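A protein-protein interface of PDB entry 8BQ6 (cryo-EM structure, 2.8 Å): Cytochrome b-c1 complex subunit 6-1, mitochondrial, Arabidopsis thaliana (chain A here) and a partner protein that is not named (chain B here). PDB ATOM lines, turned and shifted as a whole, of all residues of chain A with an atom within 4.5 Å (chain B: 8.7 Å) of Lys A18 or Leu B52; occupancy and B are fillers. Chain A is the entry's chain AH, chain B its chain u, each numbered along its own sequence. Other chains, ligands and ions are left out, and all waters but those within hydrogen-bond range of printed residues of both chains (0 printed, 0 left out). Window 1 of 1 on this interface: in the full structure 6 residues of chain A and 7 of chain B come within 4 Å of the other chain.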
ATOM      1  N   GLU A  14      -9.042  24.499  -3.362  1.00  0.00           N
ATOM      2  CA  GLU A  14      -9.538  23.347  -4.169  1.00  0.00           C
ATOM      3  C   GLU A  14      -8.659  23.167  -5.406  1.00  0.00           C
ATOM      4  O   GLU A  14      -8.539  22.024  -5.874  1.00  0.00           O
ATOM      5  CB  GLU A  14     -10.996  23.549  -4.590  1.00  0.00           C
ATOM      6  CG  GLU A  14     -12.005  23.088  -3.555  1.00  0.00           C
ATOM      7  CD  GLU A  14     -13.406  23.662  -3.699  1.00  0.00           C
ATOM      8  OE1 GLU A  14     -13.606  24.544  -4.557  1.00  0.00           O
ATOM      9  OE2 GLU A  14     -14.298  23.226  -2.947  1.00  0.00           O
ATOM     10  N   GLU A  15      -8.104  24.257  -5.932  1.00  0.00           N
ATOM     11  CA  GLU A  15      -7.166  24.149  -7.075  1.00  0.00           C
ATOM     12  C   GLU A  15      -5.783  23.761  -6.536  1.00  0.00           C
ATOM     13  O   GLU A  15      -5.079  23.027  -7.242  1.00  0.00           O
ATOM     14  CB  GLU A  15      -7.138  25.451  -7.870  1.00  0.00           C
ATOM     15  CG  GLU A  15      -6.659  25.288  -9.299  1.00  0.00           C
ATOM     16  CD  GLU A  15      -7.728  24.920 -10.314  1.00  0.00           C
ATOM     17  OE1 GLU A  15      -8.899  24.752  -9.914  1.00  0.00           O
ATOM     18  OE2 GLU A  15      -7.386  24.804 -11.509  1.00  0.00           O
ATOM     19  N   SER A  16      -5.419  24.210  -5.332  1.00  0.00           N
ATOM     20  CA  SER A  16      -4.077  23.899  -4.860  1.00  0.00           C
ATOM     21  C   SER A  16      -3.955  22.493  -4.286  1.00  0.00           C
ATOM     22  O   SER A  16      -2.832  22.014  -4.095  1.00  0.00           O
ATOM     23  CB  SER A  16      -3.633  24.927  -3.815  1.00  0.00           C
ATOM     24  OG  SER A  16      -4.195  24.665  -2.541  1.00  0.00           O
ATOM     25  N   CYS A  17      -5.075  21.809  -4.045  1.00  0.00           N
ATOM     26  CA  CYS A  17      -5.038  20.425  -3.498  1.00  0.00           C
ATOM     27  C   CYS A  17      -5.110  19.405  -4.630  1.00  0.00           C
ATOM     28  O   CYS A  17      -5.074  18.203  -4.329  1.00  0.00           O
ATOM     29  CB  CYS A  17      -6.204  20.175  -2.550  1.00  0.00           C
ATOM     30  SG  CYS A  17      -5.855  20.664  -0.840  1.00  0.00           S
ATOM     31  N   LYS A  18      -5.219  19.856  -5.881  1.00  0.00           N
ATOM     32  CA  LYS A  18      -5.364  18.908  -6.983  1.00  0.00           C
ATOM     33  C   LYS A  18      -4.208  17.926  -7.119  1.00  0.00           C
ATOM     34  O   LYS A  18      -4.469  16.767  -7.482  1.00  0.00           O
ATOM     35  CB  LYS A  18      -5.582  19.665  -8.294  1.00  0.00           C
ATOM     36  CG  LYS A  18      -7.037  19.889  -8.566  1.00  0.00           C
ATOM     37  CD  LYS A  18      -7.260  21.043  -9.492  1.00  0.00           C
ATOM     38  CE  LYS A  18      -6.889  20.678 -10.904  1.00  0.00           C
ATOM     39  NZ  LYS A  18      -7.401  21.719 -11.826  1.00  0.00           N
ATOM     40  N   PRO A  19      -2.943  18.306  -6.913  1.00  0.00           N
ATOM     41  CA  PRO A  19      -1.871  17.299  -6.958  1.00  0.00           C
ATOM     42  C   PRO A  19      -2.074  16.128  -6.010  1.00  0.00           C
ATOM     43  O   PRO A  19      -1.675  15.009  -6.348  1.00  0.00           O
ATOM     44  CB  PRO A  19      -0.616  18.105  -6.589  1.00  0.00           C
ATOM     45  CG  PRO A  19      -1.125  19.460  -6.145  1.00  0.00           C
ATOM     46  CD  PRO A  19      -2.378  19.663  -6.899  1.00  0.00           C
ATOM     47  N   LYS A  20      -2.662  16.343  -4.834  1.00  0.00           N
ATOM     48  CA  LYS A  20      -2.915  15.240  -3.915  1.00  0.00           C
ATOM     49  C   LYS A  20      -3.960  14.259  -4.434  1.00  0.00           C
ATOM     50  O   LYS A  20      -4.025  13.127  -3.944  1.00  0.00           O
ATOM     51  CB  LYS A  20      -3.348  15.783  -2.552  1.00  0.00           C
ATOM     52  CG  LYS A  20      -3.452  14.725  -1.474  1.00  0.00           C
ATOM     53  CD  LYS A  20      -4.068  15.266  -0.205  1.00  0.00           C
ATOM     54  CE  LYS A  20      -3.531  14.523   1.003  1.00  0.00           C
ATOM     55  NZ  LYS A  20      -3.103  13.144   0.639  1.00  0.00           N
ATOM     56  N   CYS A  21      -4.760  14.648  -5.420  1.00  0.00           N
ATOM     57  CA  CYS A  21      -5.869  13.839  -5.903  1.00  0.00           C
ATOM     58  C   CYS A  21      -5.754  13.586  -7.397  1.00  0.00           C
ATOM     59  O   CYS A  21      -6.734  13.660  -8.141  1.00  0.00           O
ATOM     60  CB  CYS A  21      -7.199  14.504  -5.565  1.00  0.00           C
ATOM     61  SG  CYS A  21      -7.377  14.859  -3.814  1.00  0.00           S
ATOM     62  N   VAL A  22      -4.540  13.287  -7.853  1.00  0.00           N
ATOM     63  CA  VAL A  22      -4.319  13.053  -9.273  1.00  0.00           C
ATOM     64  C   VAL A  22      -4.942  11.729  -9.702  1.00  0.00           C
ATOM     65  O   VAL A  22      -5.547  11.633 -10.776  1.00  0.00           O
ATOM     66  CB  VAL A  22      -2.815  13.115  -9.584  1.00  0.00           C
ATOM     67  CG1 VAL A  22      -2.518  12.498 -10.929  1.00  0.00           C
ATOM     68  CG2 VAL A  22      -2.347  14.544  -9.548  1.00  0.00           C
ATOM     69  N   TYR A  52     -13.111  11.750  -6.717  1.00  0.00           N
ATOM     70  CA  TYR A  52     -12.218  12.887  -6.894  1.00  0.00           C
ATOM     71  C   TYR A  52     -12.503  13.977  -5.870  1.00  0.00           C
ATOM     72  O   TYR A  52     -11.596  14.450  -5.177  1.00  0.00           O
ATOM     73  CB  TYR A  52     -12.344  13.432  -8.313  1.00  0.00           C
ATOM     74  CG  TYR A  52     -11.696  14.773  -8.476  1.00  0.00           C
ATOM     75  CD1 TYR A  52     -10.323  14.915  -8.365  1.00  0.00           C
ATOM     76  CD2 TYR A  52     -12.456  15.905  -8.727  1.00  0.00           C
ATOM     77  CE1 TYR A  52      -9.724  16.142  -8.508  1.00  0.00           C
ATOM     78  CE2 TYR A  52     -11.867  17.137  -8.872  1.00  0.00           C
ATOM     79  CZ  TYR A  52     -10.501  17.250  -8.761  1.00  0.00           C
ATOM     80  OH  TYR A  52      -9.908  18.479  -8.907  1.00  0.00           O
ATOM     81  N   ILE A  56     -10.522  15.621  -2.750  1.00  0.00           N
ATOM     82  CA  ILE A  56     -10.246  17.052  -2.708  1.00  0.00           C
ATOM     83  C   ILE A  56     -10.753  17.656  -1.407  1.00  0.00           C
ATOM     84  O   ILE A  56     -10.057  18.449  -0.761  1.00  0.00           O
ATOM     85  CB  ILE A  56     -10.864  17.747  -3.932  1.00  0.00           C
ATOM     86  CG1 ILE A  56     -10.046  17.427  -5.180  1.00  0.00           C
ATOM     87  CG2 ILE A  56     -10.990  19.245  -3.694  1.00  0.00           C
ATOM     88  CD1 ILE A  56      -8.829  18.276  -5.332  1.00  0.00           C
ATOM     89  N   VAL B  45       0.620   9.171 -13.779  1.00  0.00           N
ATOM     90  CA  VAL B  45       0.128   9.839 -12.542  1.00  0.00           C
ATOM     91  C   VAL B  45       1.254  10.755 -12.071  1.00  0.00           C
ATOM     92  O   VAL B  45       0.975  11.937 -11.873  1.00  0.00           O
ATOM     93  CB  VAL B  45      -0.301   8.824 -11.465  1.00  0.00           C
ATOM     94  CG1 VAL B  45      -0.353   9.439 -10.075  1.00  0.00           C
ATOM     95  CG2 VAL B  45      -1.631   8.175 -11.802  1.00  0.00           C
ATOM     96  N   ARG B  46       2.487  10.245 -12.030  1.00  0.00           N
ATOM     97  CA  ARG B  46       3.653  11.054 -11.578  1.00  0.00           C
ATOM     98  C   ARG B  46       3.871  12.263 -12.497  1.00  0.00           C
ATOM     99  O   ARG B  46       4.331  13.292 -11.981  1.00  0.00           O
ATOM    100  CB  ARG B  46       4.912  10.186 -11.493  1.00  0.00           C
ATOM    101  CG  ARG B  46       4.844   9.127 -10.402  1.00  0.00           C
ATOM    102  CD  ARG B  46       6.123   8.319 -10.315  1.00  0.00           C
ATOM    103  NE  ARG B  46       6.082   7.247  -9.331  1.00  0.00           N
ATOM    104  CZ  ARG B  46       7.041   6.342  -9.160  1.00  0.00           C
ATOM    105  NH1 ARG B  46       8.123   6.367  -9.917  1.00  0.00           N
ATOM    106  NH2 ARG B  46       6.913   5.409  -8.234  1.00  0.00           N
ATOM    107  N   ARG B  47       3.572  12.137 -13.793  1.00  0.00           N
ATOM    108  CA  ARG B  47       3.709  13.272 -14.741  1.00  0.00           C
ATOM    109  C   ARG B  47       2.620  14.304 -14.450  1.00  0.00           C
ATOM    110  O   ARG B  47       2.982  15.424 -14.053  1.00  0.00           O
ATOM    111  CB  ARG B  47       3.593  12.789 -16.189  1.00  0.00           C
ATOM    112  CG  ARG B  47       4.214  13.733 -17.206  1.00  0.00           C
ATOM    113  CD  ARG B  47       3.269  14.020 -18.355  1.00  0.00           C
ATOM    114  NE  ARG B  47       2.266  15.014 -18.002  1.00  0.00           N
ATOM    115  CZ  ARG B  47       0.958  14.872 -18.191  1.00  0.00           C
ATOM    116  NH1 ARG B  47       0.477  13.765 -18.733  1.00  0.00           N
ATOM    117  NH2 ARG B  47       0.134  15.841 -17.833  1.00  0.00           N
ATOM    118  N   VAL B  48       1.352  13.946 -14.683  1.00  0.00           N
ATOM    119  CA  VAL B  48       0.213  14.845 -14.346  1.00  0.00           C
ATOM    120  C   VAL B  48       0.488  15.482 -12.978  1.00  0.00           C
ATOM    121  O   VAL B  48       0.219  16.679 -12.833  1.00  0.00           O
ATOM    122  CB  VAL B  48      -1.106  14.053 -14.358  1.00  0.00           C
ATOM    123  CG1 VAL B  48      -2.304  14.927 -14.018  1.00  0.00           C
ATOM    124  CG2 VAL B  48      -1.329  13.364 -15.693  1.00  0.00           C
ATOM    125  N   ARG B  49       1.069  14.728 -12.039  1.00  0.00           N
ATOM    126  CA  ARG B  49       1.355  15.242 -10.671  1.00  0.00           C
ATOM    127  C   ARG B  49       2.416  16.339 -10.703  1.00  0.00           C
ATOM    128  O   ARG B  49       2.109  17.451 -10.255  1.00  0.00           O
ATOM    129  CB  ARG B  49       1.863  14.120  -9.767  1.00  0.00           C
ATOM    130  CG  ARG B  49       2.181  14.548  -8.343  1.00  0.00           C
ATOM    131  CD  ARG B  49       2.465  13.317  -7.509  1.00  0.00           C
ATOM    132  NE  ARG B  49       1.230  12.603  -7.229  1.00  0.00           N
ATOM    133  CZ  ARG B  49       1.131  11.547  -6.436  1.00  0.00           C
ATOM    134  NH1 ARG B  49       2.206  11.061  -5.837  1.00  0.00           N
ATOM    135  NH2 ARG B  49      -0.045  10.977  -6.244  1.00  0.00           N
ATOM    136  N   ALA B  50       3.624  16.036 -11.185  1.00  0.00           N
ATOM    137  CA  ALA B  50       4.712  17.043 -11.133  1.00  0.00           C
ATOM    138  C   ALA B  50       4.331  18.272 -11.970  1.00  0.00           C
ATOM    139  O   ALA B  50       4.673  19.384 -11.542  1.00  0.00           O
ATOM    140  CB  ALA B  50       6.019  16.434 -11.563  1.00  0.00           C
ATOM    141  N   GLU B  51       3.625  18.079 -13.089  1.00  0.00           N
ATOM    142  CA  GLU B  51       3.174  19.210 -13.945  1.00  0.00           C
ATOM    143  C   GLU B  51       2.215  20.111 -13.153  1.00  0.00           C
ATOM    144  O   GLU B  51       2.388  21.339 -13.218  1.00  0.00           O
ATOM    145  CB  GLU B  51       2.542  18.660 -15.225  1.00  0.00           C
ATOM    146  CG  GLU B  51       2.097  19.709 -16.231  1.00  0.00           C
ATOM    147  CD  GLU B  51       3.198  20.551 -16.857  1.00  0.00           C
ATOM    148  OE1 GLU B  51       4.376  20.176 -16.706  1.00  0.00           O
ATOM    149  OE2 GLU B  51       2.881  21.568 -17.502  1.00  0.00           O
ATOM    150  N   LEU B  52       1.260  19.520 -12.426  1.00  0.00           N
ATOM    151  CA  LEU B  52       0.274  20.294 -11.628  1.00  0.00           C
ATOM    152  C   LEU B  52       0.999  20.983 -10.481  1.00  0.00           C
ATOM    153  O   LEU B  52       0.639  22.135 -10.173  1.00  0.00           O
ATOM    154  CB  LEU B  52      -0.784  19.336 -11.070  1.00  0.00           C
ATOM    155  CG  LEU B  52      -2.173  19.410 -11.696  1.00  0.00           C
ATOM    156  CD1 LEU B  52      -2.103  19.253 -13.206  1.00  0.00           C
ATOM    157  CD2 LEU B  52      -3.080  18.348 -11.095  1.00  0.00           C
ATOM    158  N   LEU B  53       1.987  20.318  -9.881  1.00  0.00           N
ATOM    159  CA  LEU B  53       2.687  20.872  -8.689  1.00  0.00           C
ATOM    160  C   LEU B  53       3.567  22.054  -9.100  1.00  0.00           C
ATOM    161  O   LEU B  53       3.953  22.833  -8.210  1.00  0.00           O
ATOM    162  CB  LEU B  53       3.532  19.756  -8.070  1.00  0.00           C
ATOM    163  CG  LEU B  53       4.184  20.069  -6.722  1.00  0.00           C
ATOM    164  CD1 LEU B  53       4.279  18.827  -5.848  1.00  0.00           C
ATOM    165  CD2 LEU B  53       5.560  20.681  -6.919  1.00  0.00           C
ATOM    166  N   ARG B  54       3.909  22.157 -10.386  1.00  0.00           N
ATOM    167  CA  ARG B  54       4.717  23.305 -10.878  1.00  0.00           C
ATOM    168  C   ARG B  54       3.805  24.394 -11.451  1.00  0.00           C
ATOM    169  O   ARG B  54       4.318  25.501 -11.669  1.00  0.00           O
ATOM    170  CB  ARG B  54       5.745  22.849 -11.919  1.00  0.00           C
ATOM    171  CG  ARG B  54       6.737  21.809 -11.414  1.00  0.00           C
ATOM    172  CD  ARG B  54       7.868  22.284 -10.517  1.00  0.00           C
ATOM    173  NE  ARG B  54       7.460  22.772  -9.204  1.00  0.00           N
ATOM    174  CZ  ARG B  54       7.146  22.017  -8.154  1.00  0.00           C
ATOM    175  NH1 ARG B  54       7.192  20.698  -8.230  1.00  0.00           N
ATOM    176  NH2 ARG B  54       6.781  22.594  -7.024  1.00  0.00           N
ATOM    177  N   LYS B  55       2.518  24.107 -11.696  1.00  0.00           N
ATOM    178  CA  LYS B  55       1.670  25.200 -12.159  1.00  0.00           C
ATOM    179  C   LYS B  55       1.667  26.356 -11.165  1.00  0.00           C
ATOM    180  O   LYS B  55       1.577  27.524 -11.561  1.00  0.00           O
ATOM    181  CB  LYS B  55       0.257  24.681 -12.410  1.00  0.00           C
ATOM    182  CG  LYS B  55      -0.707  25.718 -12.934  1.00  0.00           C
ATOM    183  CD  LYS B  55      -0.407  26.117 -14.361  1.00  0.00           C
ATOM    184  CE  LYS B  55      -1.519  27.006 -14.875  1.00  0.00           C
ATOM    185  NZ  LYS B  55      -2.794  26.238 -14.915  1.00  0.00           N
ATOM    186  N   ALA B  56       1.772  26.053  -9.874  1.00  0.00           N
ATOM    187  CA  ALA B  56       1.964  27.081  -8.855  1.00  0.00           C
ATOM    188  C   ALA B  56       3.449  27.248  -8.534  1.00  0.00           C
ATOM    189  O   ALA B  56       4.228  27.736  -9.355  1.00  0.00           O
ATOM    190  CB  ALA B  56       1.183  26.739  -7.592  1.00  0.00           C
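The side-chain carboxylate (OE2) of Glu A15 is in salt-bridge range of the side-chain amino group (NZ) of Lys A18, at 3.1 Å.
Among the printed residues, pairs that only touch across the chains: Lys A18 with Leu B52 (3.98 Å), Pro A19 with Arg B49 (3.9 Å), Val A22 with Val B45 (3.7 Å), Val A22 with Val B48 (3.9 Å) and Val A22 with Arg B49 (3.9 Å).
Of chain B, only Leu B52 comes within 4 Å of Lys A18. Of the printed residues of chain B, Val A22 touches Val B45 (3.7 Å), Val B48 (3.9 Å) and Arg B49 (3.9 Å). Of the printed residues of chain A, Val B48 touches Val A22. Printed residues of chain A within 4 Å of Arg B49: Pro A19 (3.9 Å) and Val A22 (3.9 Å). Of the printed residues of chain A, Val B45 touches Val A22. Lys A20 touches none of the printed residues of chain B. Arg B54 touches none of the printed residues of chain A. The nearest residue of chain B that does not touch Lys A18 is Arg B49 (6.8 Å). The nearest printed residue of chain A that does not touch Leu B52 is Val A22 (4.2 Å).
Of the 12 printed residues of chain B, 4 touch a printed residue of chain A. Hydrophobic or aromatic side chains of chain B within 4 Å of the printed part of chain A: Val B45, Val B48 and Leu B52. Of the 11 printed residues of chain A, 3 touch a printed residue of chain B. Printed residues of chain A that touch a printed residue of chain B: Lys A18, Pro A19 and Val A22. Hydrophobic or aromatic side chains of chain A within 4 Å of the printed part of chain B: Val A22. Among the printed residues, 5 pairs touch across the chains. Among the printed residues, no Asp or Glu carboxylate lies within 4 Å of a Lys or Arg side-chain nitrogen of the other chain.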
